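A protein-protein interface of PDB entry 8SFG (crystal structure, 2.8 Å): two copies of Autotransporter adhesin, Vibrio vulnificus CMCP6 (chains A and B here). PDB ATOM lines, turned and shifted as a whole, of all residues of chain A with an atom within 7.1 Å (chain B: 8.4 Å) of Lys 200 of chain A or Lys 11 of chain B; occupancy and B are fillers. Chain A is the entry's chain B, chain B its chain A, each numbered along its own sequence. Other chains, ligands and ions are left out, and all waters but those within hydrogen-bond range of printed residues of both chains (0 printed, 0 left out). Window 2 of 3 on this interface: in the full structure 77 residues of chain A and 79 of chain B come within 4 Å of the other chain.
The backbone carbonyl oxygen (O) of Lys 200 of chain A lies within hydrogen-bond range of the side-chain hydroxyl (OH) of Tyr 327 of chain A (2.7 Å).
Of the 16 printed residues of chain B, 4 touch a printed residue of chain A.
Hydrophobic or aromatic side chains of chain B within 4 Å of the printed part of chain A: Phe 10.
Printed residues of chain A that touch a printed residue of chain B: Ala 195, His 198, Ala 199, Lys 200, Thr 330 and Phe 331.
Hydrophobic or aromatic side chains of chain A within 4 Å of the printed part of chain B: Ala 195, His 198 and Ala 199.
Among the printed residues, 7 pairs touch across the chains.
No position is printed for both chains.
Of the 7 pairs that touch across the chains among the printed residues, none has its exchanged pair printed and touching as well.
Among the printed residues, merely in contact across the chains: Phe 331 of chain A with Lys 18 of chain B, Ala 195 of chain A with Phe 10 of chain B, Ala 199 of chain A with Lys 11 of chain B and Thr 330 of chain A with Lys 18 of chain B.
Of the printed residues of chain B, Ala 195 of chain A touches Phe 10.
Printed residues of chain B within 4 Å of His 198 of chain A: Glu 7.
Ala 199 of chain A touches just these residues of chain B: Glu 7 (3.1 Å) and Lys 11 (3.8 Å).
Pro 202 of chain A touches none of the printed residues of chain B.
Of the printed residues of chain B, Thr 330 of chain A touches Lys 18.
Of the printed residues of chain B, Phe 331 of chain A touches Lys 18.
Of chain A, only Ala 199 (3.8 Å) and Lys 200 (3.4 Å) come within 4 Å of Lys 11 of chain B.
Tyr 13 of chain B touches none of the printed residues of chain A.
The nearest residue of chain B that does not touch Lys 200 of chain A is Glu 7 of chain B (4.9 Å).
The nearest residue of chain A that does not touch Lys 11 of chain B is His 198 of chain A (6.4 Å).
The nearest printed residue of chain B that does not touch Ala 195 of chain A is Glu 7 of chain B (6.0 Å).
O of Ala 199 of chain A sits close to OE2 of Glu 7 of chain B (3.4 Å).
The side-chain amino group (NZ) of Lys 200 of chain A lies close to the side-chain amino group (NZ) of Lys 11 of chain B (3.4 Å).
O of His 198 of chain A lies close to OE2 of Glu 7 of chain B.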
ATOM      1  N   ALA A 195      -3.649 -18.295 -30.185  1.00  0.00           N
ATOM      2  CA  ALA A 195      -4.121 -19.005 -28.973  1.00  0.00           C
ATOM      3  C   ALA A 195      -3.674 -18.241 -27.723  1.00  0.00           C
ATOM      4  O   ALA A 195      -4.392 -18.303 -26.706  1.00  0.00           O
ATOM      5  CB  ALA A 195      -3.597 -20.420 -28.961  1.00  0.00           C
ATOM      6  N   ALA A 196      -2.526 -17.559 -27.805  1.00  0.00           N
ATOM      7  CA  ALA A 196      -1.986 -16.786 -26.664  1.00  0.00           C
ATOM      8  C   ALA A 196      -2.895 -15.584 -26.388  1.00  0.00           C
ATOM      9  O   ALA A 196      -3.206 -15.345 -25.205  1.00  0.00           O
ATOM     10  CB  ALA A 196      -0.570 -16.356 -26.955  1.00  0.00           C
ATOM     11  N   ILE A 197      -3.296 -14.872 -27.449  1.00  0.00           N
ATOM     12  CA  ILE A 197      -4.188 -13.675 -27.347  1.00  0.00           C
ATOM     13  C   ILE A 197      -5.509 -14.091 -26.684  1.00  0.00           C
ATOM     14  O   ILE A 197      -6.106 -13.253 -25.991  1.00  0.00           O
ATOM     15  CB  ILE A 197      -4.417 -13.043 -28.738  1.00  0.00           C
ATOM     16  CG1 ILE A 197      -3.092 -12.662 -29.404  1.00  0.00           C
ATOM     17  CG2 ILE A 197      -5.366 -11.852 -28.646  1.00  0.00           C
ATOM     18  CD1 ILE A 197      -3.228 -12.133 -30.812  1.00  0.00           C
ATOM     19  N   HIS A 198      -5.943 -15.335 -26.894  1.00  0.00           N
ATOM     20  CA  HIS A 198      -7.210 -15.815 -26.285  1.00  0.00           C
ATOM     21  C   HIS A 198      -6.960 -16.219 -24.827  1.00  0.00           C
ATOM     22  O   HIS A 198      -7.798 -15.885 -23.967  1.00  0.00           O
ATOM     23  CB  HIS A 198      -7.819 -16.955 -27.113  1.00  0.00           C
ATOM     24  CG  HIS A 198      -9.074 -17.494 -26.520  1.00  0.00           C
ATOM     25  ND1 HIS A 198      -9.083 -18.617 -25.721  1.00  0.00           N
ATOM     26  CD2 HIS A 198     -10.349 -17.047 -26.567  1.00  0.00           C
ATOM     27  CE1 HIS A 198     -10.312 -18.854 -25.307  1.00  0.00           C
ATOM     28  NE2 HIS A 198     -11.106 -17.902 -25.809  1.00  0.00           N
ATOM     29  N   ALA A 199      -5.848 -16.911 -24.571  1.00  0.00           N
ATOM     30  CA  ALA A 199      -5.497 -17.356 -23.202  1.00  0.00           C
ATOM     31  C   ALA A 199      -5.347 -16.136 -22.288  1.00  0.00           C
ATOM     32  O   ALA A 199      -5.873 -16.178 -21.163  1.00  0.00           O
ATOM     33  CB  ALA A 199      -4.232 -18.180 -23.235  1.00  0.00           C
ATOM     34  N   LYS A 200      -4.658 -15.097 -22.767  1.00  0.00           N
ATOM     35  CA  LYS A 200      -4.431 -13.849 -21.987  1.00  0.00           C
ATOM     36  C   LYS A 200      -5.102 -12.691 -22.733  1.00  0.00           C
ATOM     37  O   LYS A 200      -4.406 -11.950 -23.461  1.00  0.00           O
ATOM     38  CB  LYS A 200      -2.930 -13.622 -21.765  1.00  0.00           C
ATOM     39  CG  LYS A 200      -2.215 -14.795 -21.106  1.00  0.00           C
ATOM     40  CD  LYS A 200      -2.816 -15.253 -19.794  1.00  0.00           C
ATOM     41  CE  LYS A 200      -2.133 -16.493 -19.255  1.00  0.00           C
ATOM     42  NZ  LYS A 200      -2.787 -16.998 -18.025  1.00  0.00           N
ATOM     43  N   ASN A 201      -6.422 -12.573 -22.566  1.00  0.00           N
ATOM     44  CA  ASN A 201      -7.231 -11.505 -23.211  1.00  0.00           C
ATOM     45  C   ASN A 201      -6.685 -10.145 -22.781  1.00  0.00           C
ATOM     46  O   ASN A 201      -6.682  -9.834 -21.592  1.00  0.00           O
ATOM     47  CB  ASN A 201      -8.712 -11.654 -22.851  1.00  0.00           C
ATOM     48  CG  ASN A 201      -9.596 -10.612 -23.499  1.00  0.00           C
ATOM     49  OD1 ASN A 201      -9.178  -9.927 -24.436  1.00  0.00           O
ATOM     50  ND2 ASN A 201     -10.823 -10.496 -23.017  1.00  0.00           N
ATOM     51  N   PRO A 202      -6.215  -9.288 -23.720  1.00  0.00           N
ATOM     52  CA  PRO A 202      -5.672  -7.974 -23.364  1.00  0.00           C
ATOM     53  C   PRO A 202      -6.664  -7.038 -22.674  1.00  0.00           C
ATOM     54  O   PRO A 202      -6.265  -6.032 -22.089  1.00  0.00           O
ATOM     55  CB  PRO A 202      -5.225  -7.370 -24.706  1.00  0.00           C
ATOM     56  CG  PRO A 202      -5.989  -8.162 -25.758  1.00  0.00           C
ATOM     57  CD  PRO A 202      -6.158  -9.545 -25.167  1.00  0.00           C
ATOM     58  N   MET A 203      -7.955  -7.387 -22.732  1.00  0.00           N
ATOM     59  CA  MET A 203      -8.993  -6.578 -22.111  1.00  0.00           C
ATOM     60  C   MET A 203      -8.904  -6.671 -20.588  1.00  0.00           C
ATOM     61  O   MET A 203      -9.380  -5.776 -19.893  1.00  0.00           O
ATOM     62  CB  MET A 203     -10.377  -7.036 -22.580  1.00  0.00           C
ATOM     63  CG  MET A 203     -10.641  -6.832 -24.067  1.00  0.00           C
ATOM     64  SD  MET A 203     -10.731  -4.940 -24.555  1.00  0.00           S
ATOM     65  CE  MET A 203     -12.118  -4.086 -23.454  1.00  0.00           C
ATOM     66  N   HIS A 204      -8.291  -7.747 -20.076  1.00  0.00           N
ATOM     67  CA  HIS A 204      -8.165  -7.943 -18.638  1.00  0.00           C
ATOM     68  C   HIS A 204      -6.794  -7.491 -18.120  1.00  0.00           C
ATOM     69  O   HIS A 204      -6.578  -7.585 -16.895  1.00  0.00           O
ATOM     70  CB  HIS A 204      -8.408  -9.412 -18.268  1.00  0.00           C
ATOM     71  CG  HIS A 204      -9.761  -9.916 -18.638  1.00  0.00           C
ATOM     72  ND1 HIS A 204      -9.971 -10.692 -19.761  1.00  0.00           N
ATOM     73  CD2 HIS A 204     -10.967  -9.746 -18.056  1.00  0.00           C
ATOM     74  CE1 HIS A 204     -11.250 -10.991 -19.849  1.00  0.00           C
ATOM     75  NE2 HIS A 204     -11.886 -10.415 -18.814  1.00  0.00           N
ATOM     76  N   ASP A 205      -5.900  -7.030 -18.998  1.00  0.00           N
ATOM     77  CA  ASP A 205      -4.553  -6.580 -18.551  1.00  0.00           C
ATOM     78  C   ASP A 205      -4.715  -5.334 -17.667  1.00  0.00           C
ATOM     79  O   ASP A 205      -5.558  -4.479 -17.992  1.00  0.00           O
ATOM     80  CB  ASP A 205      -3.631  -6.359 -19.753  1.00  0.00           C
ATOM     81  CG  ASP A 205      -2.216  -5.963 -19.379  1.00  0.00           C
ATOM     82  OD1 ASP A 205      -2.007  -5.545 -18.238  1.00  0.00           O
ATOM     83  OD2 ASP A 205      -1.326  -6.104 -20.228  1.00  0.00           O
ATOM     84  N   TYR A 327       0.801  -4.394 -27.108  1.00  0.00           N
ATOM     85  CA  TYR A 327       0.481  -5.433 -26.090  1.00  0.00           C
ATOM     86  C   TYR A 327       1.220  -6.744 -26.408  1.00  0.00           C
ATOM     87  O   TYR A 327       1.320  -7.116 -27.587  1.00  0.00           O
ATOM     88  CB  TYR A 327      -1.027  -5.660 -26.008  1.00  0.00           C
ATOM     89  CG  TYR A 327      -1.428  -6.836 -25.153  1.00  0.00           C
ATOM     90  CD1 TYR A 327      -1.467  -6.742 -23.773  1.00  0.00           C
ATOM     91  CD2 TYR A 327      -1.780  -8.046 -25.727  1.00  0.00           C
ATOM     92  CE1 TYR A 327      -1.839  -7.822 -22.986  1.00  0.00           C
ATOM     93  CE2 TYR A 327      -2.153  -9.134 -24.955  1.00  0.00           C
ATOM     94  CZ  TYR A 327      -2.183  -9.022 -23.578  1.00  0.00           C
ATOM     95  OH  TYR A 327      -2.548 -10.088 -22.812  1.00  0.00           O
ATOM     96  N   LYS A 328       1.715  -7.419 -25.364  1.00  0.00           N
ATOM     97  CA  LYS A 328       2.445  -8.709 -25.490  1.00  0.00           C
ATOM     98  C   LYS A 328       1.563  -9.826 -24.939  1.00  0.00           C
ATOM     99  O   LYS A 328       1.374  -9.917 -23.728  1.00  0.00           O
ATOM    100  CB  LYS A 328       3.772  -8.642 -24.734  1.00  0.00           C
ATOM    101  CG  LYS A 328       4.724  -7.550 -25.199  1.00  0.00           C
ATOM    102  CD  LYS A 328       6.049  -7.542 -24.461  1.00  0.00           C
ATOM    103  CE  LYS A 328       6.974  -6.442 -24.940  1.00  0.00           C
ATOM    104  NZ  LYS A 328       6.388  -5.096 -24.725  1.00  0.00           N
ATOM    105  N   PRO A 329       0.989 -10.702 -25.798  1.00  0.00           N
ATOM    106  CA  PRO A 329       0.118 -11.787 -25.338  1.00  0.00           C
ATOM    107  C   PRO A 329       0.796 -12.885 -24.504  1.00  0.00           C
ATOM    108  O   PRO A 329       0.210 -13.304 -23.516  1.00  0.00           O
ATOM    109  CB  PRO A 329      -0.414 -12.417 -26.638  1.00  0.00           C
ATOM    110  CG  PRO A 329      -0.152 -11.370 -27.702  1.00  0.00           C
ATOM    111  CD  PRO A 329       1.113 -10.675 -27.260  1.00  0.00           C
ATOM    112  N   THR A 330       1.985 -13.327 -24.923  1.00  0.00           N
ATOM    113  CA  THR A 330       2.721 -14.405 -24.198  1.00  0.00           C
ATOM    114  C   THR A 330       3.771 -13.778 -23.271  1.00  0.00           C
ATOM    115  O   THR A 330       4.695 -13.115 -23.781  1.00  0.00           O
ATOM    116  CB  THR A 330       3.312 -15.430 -25.180  1.00  0.00           C
ATOM    117  OG1 THR A 330       4.074 -16.381 -24.435  1.00  0.00           O
ATOM    118  CG2 THR A 330       4.163 -14.801 -26.259  1.00  0.00           C
ATOM    119  N   PHE A 331       3.621 -13.990 -21.957  1.00  0.00           N
ATOM    120  CA  PHE A 331       4.564 -13.454 -20.934  1.00  0.00           C
ATOM    121  C   PHE A 331       5.961 -14.031 -21.186  1.00  0.00           C
ATOM    122  O   PHE A 331       6.065 -15.174 -21.674  1.00  0.00           O
ATOM    123  CB  PHE A 331       4.074 -13.783 -19.518  1.00  0.00           C
ATOM    124  CG  PHE A 331       4.975 -13.299 -18.407  1.00  0.00           C
ATOM    125  CD1 PHE A 331       4.846 -12.017 -17.891  1.00  0.00           C
ATOM    126  CD2 PHE A 331       5.958 -14.123 -17.878  1.00  0.00           C
ATOM    127  CE1 PHE A 331       5.682 -11.571 -16.877  1.00  0.00           C
ATOM    128  CE2 PHE A 331       6.796 -13.675 -16.865  1.00  0.00           C
ATOM    129  CZ  PHE A 331       6.654 -12.401 -16.365  1.00  0.00           C
ATOM    130  N   GLY B   5     -12.545 -27.469 -22.124  1.00  0.00           N
ATOM    131  CA  GLY B   5     -11.395 -26.968 -21.386  1.00  0.00           C
ATOM    132  C   GLY B   5     -10.102 -27.093 -22.179  1.00  0.00           C
ATOM    133  O   GLY B   5      -9.092 -27.535 -21.593  1.00  0.00           O
ATOM    134  N   LEU B   6     -10.135 -26.706 -23.458  1.00  0.00           N
ATOM    135  CA  LEU B   6      -8.956 -26.773 -24.367  1.00  0.00           C
ATOM    136  C   LEU B   6      -7.973 -25.638 -24.051  1.00  0.00           C
ATOM    137  O   LEU B   6      -6.777 -25.786 -24.374  1.00  0.00           O
ATOM    138  CB  LEU B   6      -9.450 -26.677 -25.815  1.00  0.00           C
ATOM    139  CG  LEU B   6      -8.358 -26.609 -26.880  1.00  0.00           C
ATOM    140  CD1 LEU B   6      -7.393 -27.776 -26.747  1.00  0.00           C
ATOM    141  CD2 LEU B   6      -8.960 -26.569 -28.275  1.00  0.00           C
ATOM    142  N   GLU B   7      -8.465 -24.550 -23.451  1.00  0.00           N
ATOM    143  CA  GLU B   7      -7.607 -23.381 -23.114  1.00  0.00           C
ATOM    144  C   GLU B   7      -6.638 -23.770 -21.989  1.00  0.00           C
ATOM    145  O   GLU B   7      -5.437 -23.456 -22.130  1.00  0.00           O
ATOM    146  CB  GLU B   7      -8.492 -22.186 -22.759  1.00  0.00           C
ATOM    147  CG  GLU B   7      -7.726 -20.902 -22.511  1.00  0.00           C
ATOM    148  CD  GLU B   7      -8.613 -19.689 -22.278  1.00  0.00           C
ATOM    149  OE1 GLU B   7      -9.850 -19.833 -22.358  1.00  0.00           O
ATOM    150  OE2 GLU B   7      -8.068 -18.601 -22.019  1.00  0.00           O
ATOM    151  N   LYS B   8      -7.140 -24.423 -20.929  1.00  0.00           N
ATOM    152  CA  LYS B   8      -6.299 -24.882 -19.781  1.00  0.00           C
ATOM    153  C   LYS B   8      -5.321 -25.974 -20.237  1.00  0.00           C
ATOM    154  O   LYS B   8      -4.213 -26.060 -19.661  1.00  0.00           O
ATOM    155  CB  LYS B   8      -7.174 -25.407 -18.635  1.00  0.00           C
ATOM    156  CG  LYS B   8      -7.772 -24.355 -17.713  1.00  0.00           C
ATOM    157  CD  LYS B   8      -6.726 -23.683 -16.849  1.00  0.00           C
ATOM    158  CE  LYS B   8      -7.303 -22.725 -15.829  1.00  0.00           C
ATOM    159  NZ  LYS B   8      -6.233 -22.105 -15.016  1.00  0.00           N
ATOM    160  N   ASP B   9      -5.714 -26.759 -21.248  1.00  0.00           N
ATOM    161  CA  ASP B   9      -4.855 -27.851 -21.783  1.00  0.00           C
ATOM    162  C   ASP B   9      -3.729 -27.260 -22.637  1.00  0.00           C
ATOM    163  O   ASP B   9      -2.665 -27.890 -22.707  1.00  0.00           O
ATOM    164  CB  ASP B   9      -5.677 -28.870 -22.577  1.00  0.00           C
ATOM    165  CG  ASP B   9      -6.688 -29.632 -21.731  1.00  0.00           C
ATOM    166  OD1 ASP B   9      -6.648 -29.480 -20.494  1.00  0.00           O
ATOM    167  OD2 ASP B   9      -7.516 -30.357 -22.311  1.00  0.00           O
ATOM    168  N   PHE B  10      -3.954 -26.097 -23.258  1.00  0.00           N
ATOM    169  CA  PHE B  10      -2.909 -25.469 -24.109  1.00  0.00           C
ATOM    170  C   PHE B  10      -1.917 -24.685 -23.233  1.00  0.00           C
ATOM    171  O   PHE B  10      -0.734 -24.595 -23.627  1.00  0.00           O
ATOM    172  CB  PHE B  10      -3.542 -24.597 -25.197  1.00  0.00           C
ATOM    173  CG  PHE B  10      -2.555 -24.094 -26.220  1.00  0.00           C
ATOM    174  CD1 PHE B  10      -2.205 -24.885 -27.307  1.00  0.00           C
ATOM    175  CD2 PHE B  10      -1.969 -22.843 -26.095  1.00  0.00           C
ATOM    176  CE1 PHE B  10      -1.282 -24.439 -28.238  1.00  0.00           C
ATOM    177  CE2 PHE B  10      -1.057 -22.393 -27.038  1.00  0.00           C
ATOM    178  CZ  PHE B  10      -0.722 -23.188 -28.113  1.00  0.00           C
ATOM    179  N   LYS B  11      -2.373 -24.138 -22.096  1.00  0.00           N
ATOM    180  CA  LYS B  11      -1.469 -23.382 -21.181  1.00  0.00           C
ATOM    181  C   LYS B  11      -0.468 -24.349 -20.534  1.00  0.00           C
ATOM    182  O   LYS B  11       0.726 -23.997 -20.457  1.00  0.00           O
ATOM    183  CB  LYS B  11      -2.246 -22.647 -20.082  1.00  0.00           C
ATOM    184  CG  LYS B  11      -3.131 -21.495 -20.537  1.00  0.00           C
ATOM    185  CD  LYS B  11      -3.849 -20.830 -19.376  1.00  0.00           C
ATOM    186  CE  LYS B  11      -4.699 -19.645 -19.782  1.00  0.00           C
ATOM    187  NZ  LYS B  11      -5.385 -19.040 -18.616  1.00  0.00           N
ATOM    188  N   ARG B  12      -0.950 -25.514 -20.085  1.00  0.00           N
ATOM    189  CA  ARG B  12      -0.101 -26.547 -19.433  1.00  0.00           C
ATOM    190  C   ARG B  12       0.934 -27.057 -20.443  1.00  0.00           C
ATOM    191  O   ARG B  12       2.073 -27.367 -20.031  1.00  0.00           O
ATOM    192  CB  ARG B  12      -0.975 -27.718 -18.980  1.00  0.00           C
ATOM    193  CG  ARG B  12      -0.309 -28.671 -17.997  1.00  0.00           C
ATOM    194  CD  ARG B  12      -1.071 -29.981 -17.969  1.00  0.00           C
ATOM    195  NE  ARG B  12      -2.504 -29.741 -18.069  1.00  0.00           N
ATOM    196  CZ  ARG B  12      -3.412 -30.676 -18.286  1.00  0.00           C
ATOM    197  NH1 ARG B  12      -3.055 -31.941 -18.422  1.00  0.00           N
ATOM    198  NH2 ARG B  12      -4.686 -30.343 -18.376  1.00  0.00           N
ATOM    199  N   TYR B  13       0.524 -27.151 -21.714  1.00  0.00           N
ATOM    200  CA  TYR B  13       1.386 -27.615 -22.834  1.00  0.00           C
ATOM    201  C   TYR B  13       2.477 -26.576 -23.122  1.00  0.00           C
ATOM    202  O   TYR B  13       3.662 -26.955 -23.176  1.00  0.00           O
ATOM    203  CB  TYR B  13       0.516 -27.891 -24.064  1.00  0.00           C
ATOM    204  CG  TYR B  13       1.263 -28.002 -25.370  1.00  0.00           C
ATOM    205  CD1 TYR B  13       1.869 -29.181 -25.755  1.00  0.00           C
ATOM    206  CD2 TYR B  13       1.341 -26.923 -26.234  1.00  0.00           C
ATOM    207  CE1 TYR B  13       2.545 -29.286 -26.958  1.00  0.00           C
ATOM    208  CE2 TYR B  13       2.001 -27.010 -27.448  1.00  0.00           C
ATOM    209  CZ  TYR B  13       2.614 -28.196 -27.808  1.00  0.00           C
ATOM    210  OH  TYR B  13       3.277 -28.293 -28.997  1.00  0.00           O
ATOM    211  N   GLY B  14       2.078 -25.312 -23.298  1.00  0.00           N
ATOM    212  CA  GLY B  14       3.022 -24.214 -23.589  1.00  0.00           C
ATOM    213  C   GLY B  14       4.073 -24.060 -22.501  1.00  0.00           C
ATOM    214  O   GLY B  14       5.245 -23.785 -22.847  1.00  0.00           O
ATOM    215  N   ASP B  15       3.670 -24.239 -21.237  1.00  0.00           N
ATOM    216  CA  ASP B  15       4.583 -24.118 -20.069  1.00  0.00           C
ATOM    217  C   ASP B  15       5.587 -25.278 -20.064  1.00  0.00           C
ATOM    218  O   ASP B  15       6.733 -25.067 -19.600  1.00  0.00           O
ATOM    219  CB  ASP B  15       3.802 -24.103 -18.750  1.00  0.00           C
ATOM    220  CG  ASP B  15       2.824 -22.950 -18.611  1.00  0.00           C
ATOM    221  OD1 ASP B  15       2.812 -22.076 -19.501  1.00  0.00           O
ATOM    222  OD2 ASP B  15       2.080 -22.939 -17.613  1.00  0.00           O
ATOM    223  N   ALA B  16       5.181 -26.444 -20.581  1.00  0.00           N
ATOM    224  CA  ALA B  16       6.058 -27.639 -20.604  1.00  0.00           C
ATOM    225  C   ALA B  16       7.184 -27.484 -21.635  1.00  0.00           C
ATOM    226  O   ALA B  16       7.937 -28.464 -21.812  1.00  0.00           O
ATOM    227  CB  ALA B  16       5.228 -28.868 -20.879  1.00  0.00           C
ATOM    228  N   LEU B  17       7.293 -26.316 -22.287  1.00  0.00           N
ATOM    229  CA  LEU B  17       8.358 -26.079 -23.304  1.00  0.00           C
ATOM    230  C   LEU B  17       9.215 -24.868 -22.913  1.00  0.00           C
ATOM    231  O   LEU B  17       9.694 -24.157 -23.825  1.00  0.00           O
ATOM    232  CB  LEU B  17       7.721 -25.903 -24.687  1.00  0.00           C
ATOM    233  CG  LEU B  17       7.072 -27.156 -25.276  1.00  0.00           C
ATOM    234  CD1 LEU B  17       6.300 -26.836 -26.544  1.00  0.00           C
ATOM    235  CD2 LEU B  17       8.118 -28.224 -25.549  1.00  0.00           C
ATOM    236  N   LYS B  18       9.438 -24.683 -21.608  1.00  0.00           N
ATOM    237  CA  LYS B  18      10.292 -23.582 -21.084  1.00  0.00           C
ATOM    238  C   LYS B  18      11.000 -24.060 -19.810  1.00  0.00           C
ATOM    239  O   LYS B  18      12.244 -24.110 -19.835  1.00  0.00           O
ATOM    240  CB  LYS B  18       9.466 -22.324 -20.812  1.00  0.00           C
ATOM    241  CG  LYS B  18       8.801 -21.710 -22.036  1.00  0.00           C
ATOM    242  CD  LYS B  18       8.042 -20.437 -21.734  1.00  0.00           C
ATOM    243  CE  LYS B  18       7.381 -19.836 -22.955  1.00  0.00           C
ATOM    244  NZ  LYS B  18       6.651 -18.591 -22.621  1.00  0.00           N
ATOM    245  N   VAL B  62      -2.013 -34.053 -23.950  1.00  0.00           N
ATOM    246  CA  VAL B  62      -1.216 -33.104 -23.113  1.00  0.00           C
ATOM    247  C   VAL B  62      -0.734 -33.842 -21.858  1.00  0.00           C
ATOM    248  O   VAL B  62       0.408 -33.577 -21.433  1.00  0.00           O
ATOM    249  CB  VAL B  62      -2.023 -31.834 -22.769  1.00  0.00           C
ATOM    250  CG1 VAL B  62      -1.288 -30.910 -21.803  1.00  0.00           C
ATOM    251  CG2 VAL B  62      -2.428 -31.072 -24.024  1.00  0.00           C
ATOM    252  N   VAL B  66       3.165 -33.975 -20.726  1.00  0.00           N
ATOM    253  CA  VAL B  66       3.699 -33.446 -19.432  1.00  0.00           C
ATOM    254  C   VAL B  66       4.239 -34.618 -18.600  1.00  0.00           C
ATOM    255  O   VAL B  66       5.446 -34.591 -18.257  1.00  0.00           O
ATOM    256  CB  VAL B  66       2.644 -32.628 -18.654  1.00  0.00           C
ATOM    257  CG1 VAL B  66       2.179 -31.408 -19.437  1.00  0.00           C
ATOM    258  CG2 VAL B  66       1.449 -33.466 -18.233  1.00  0.00           C
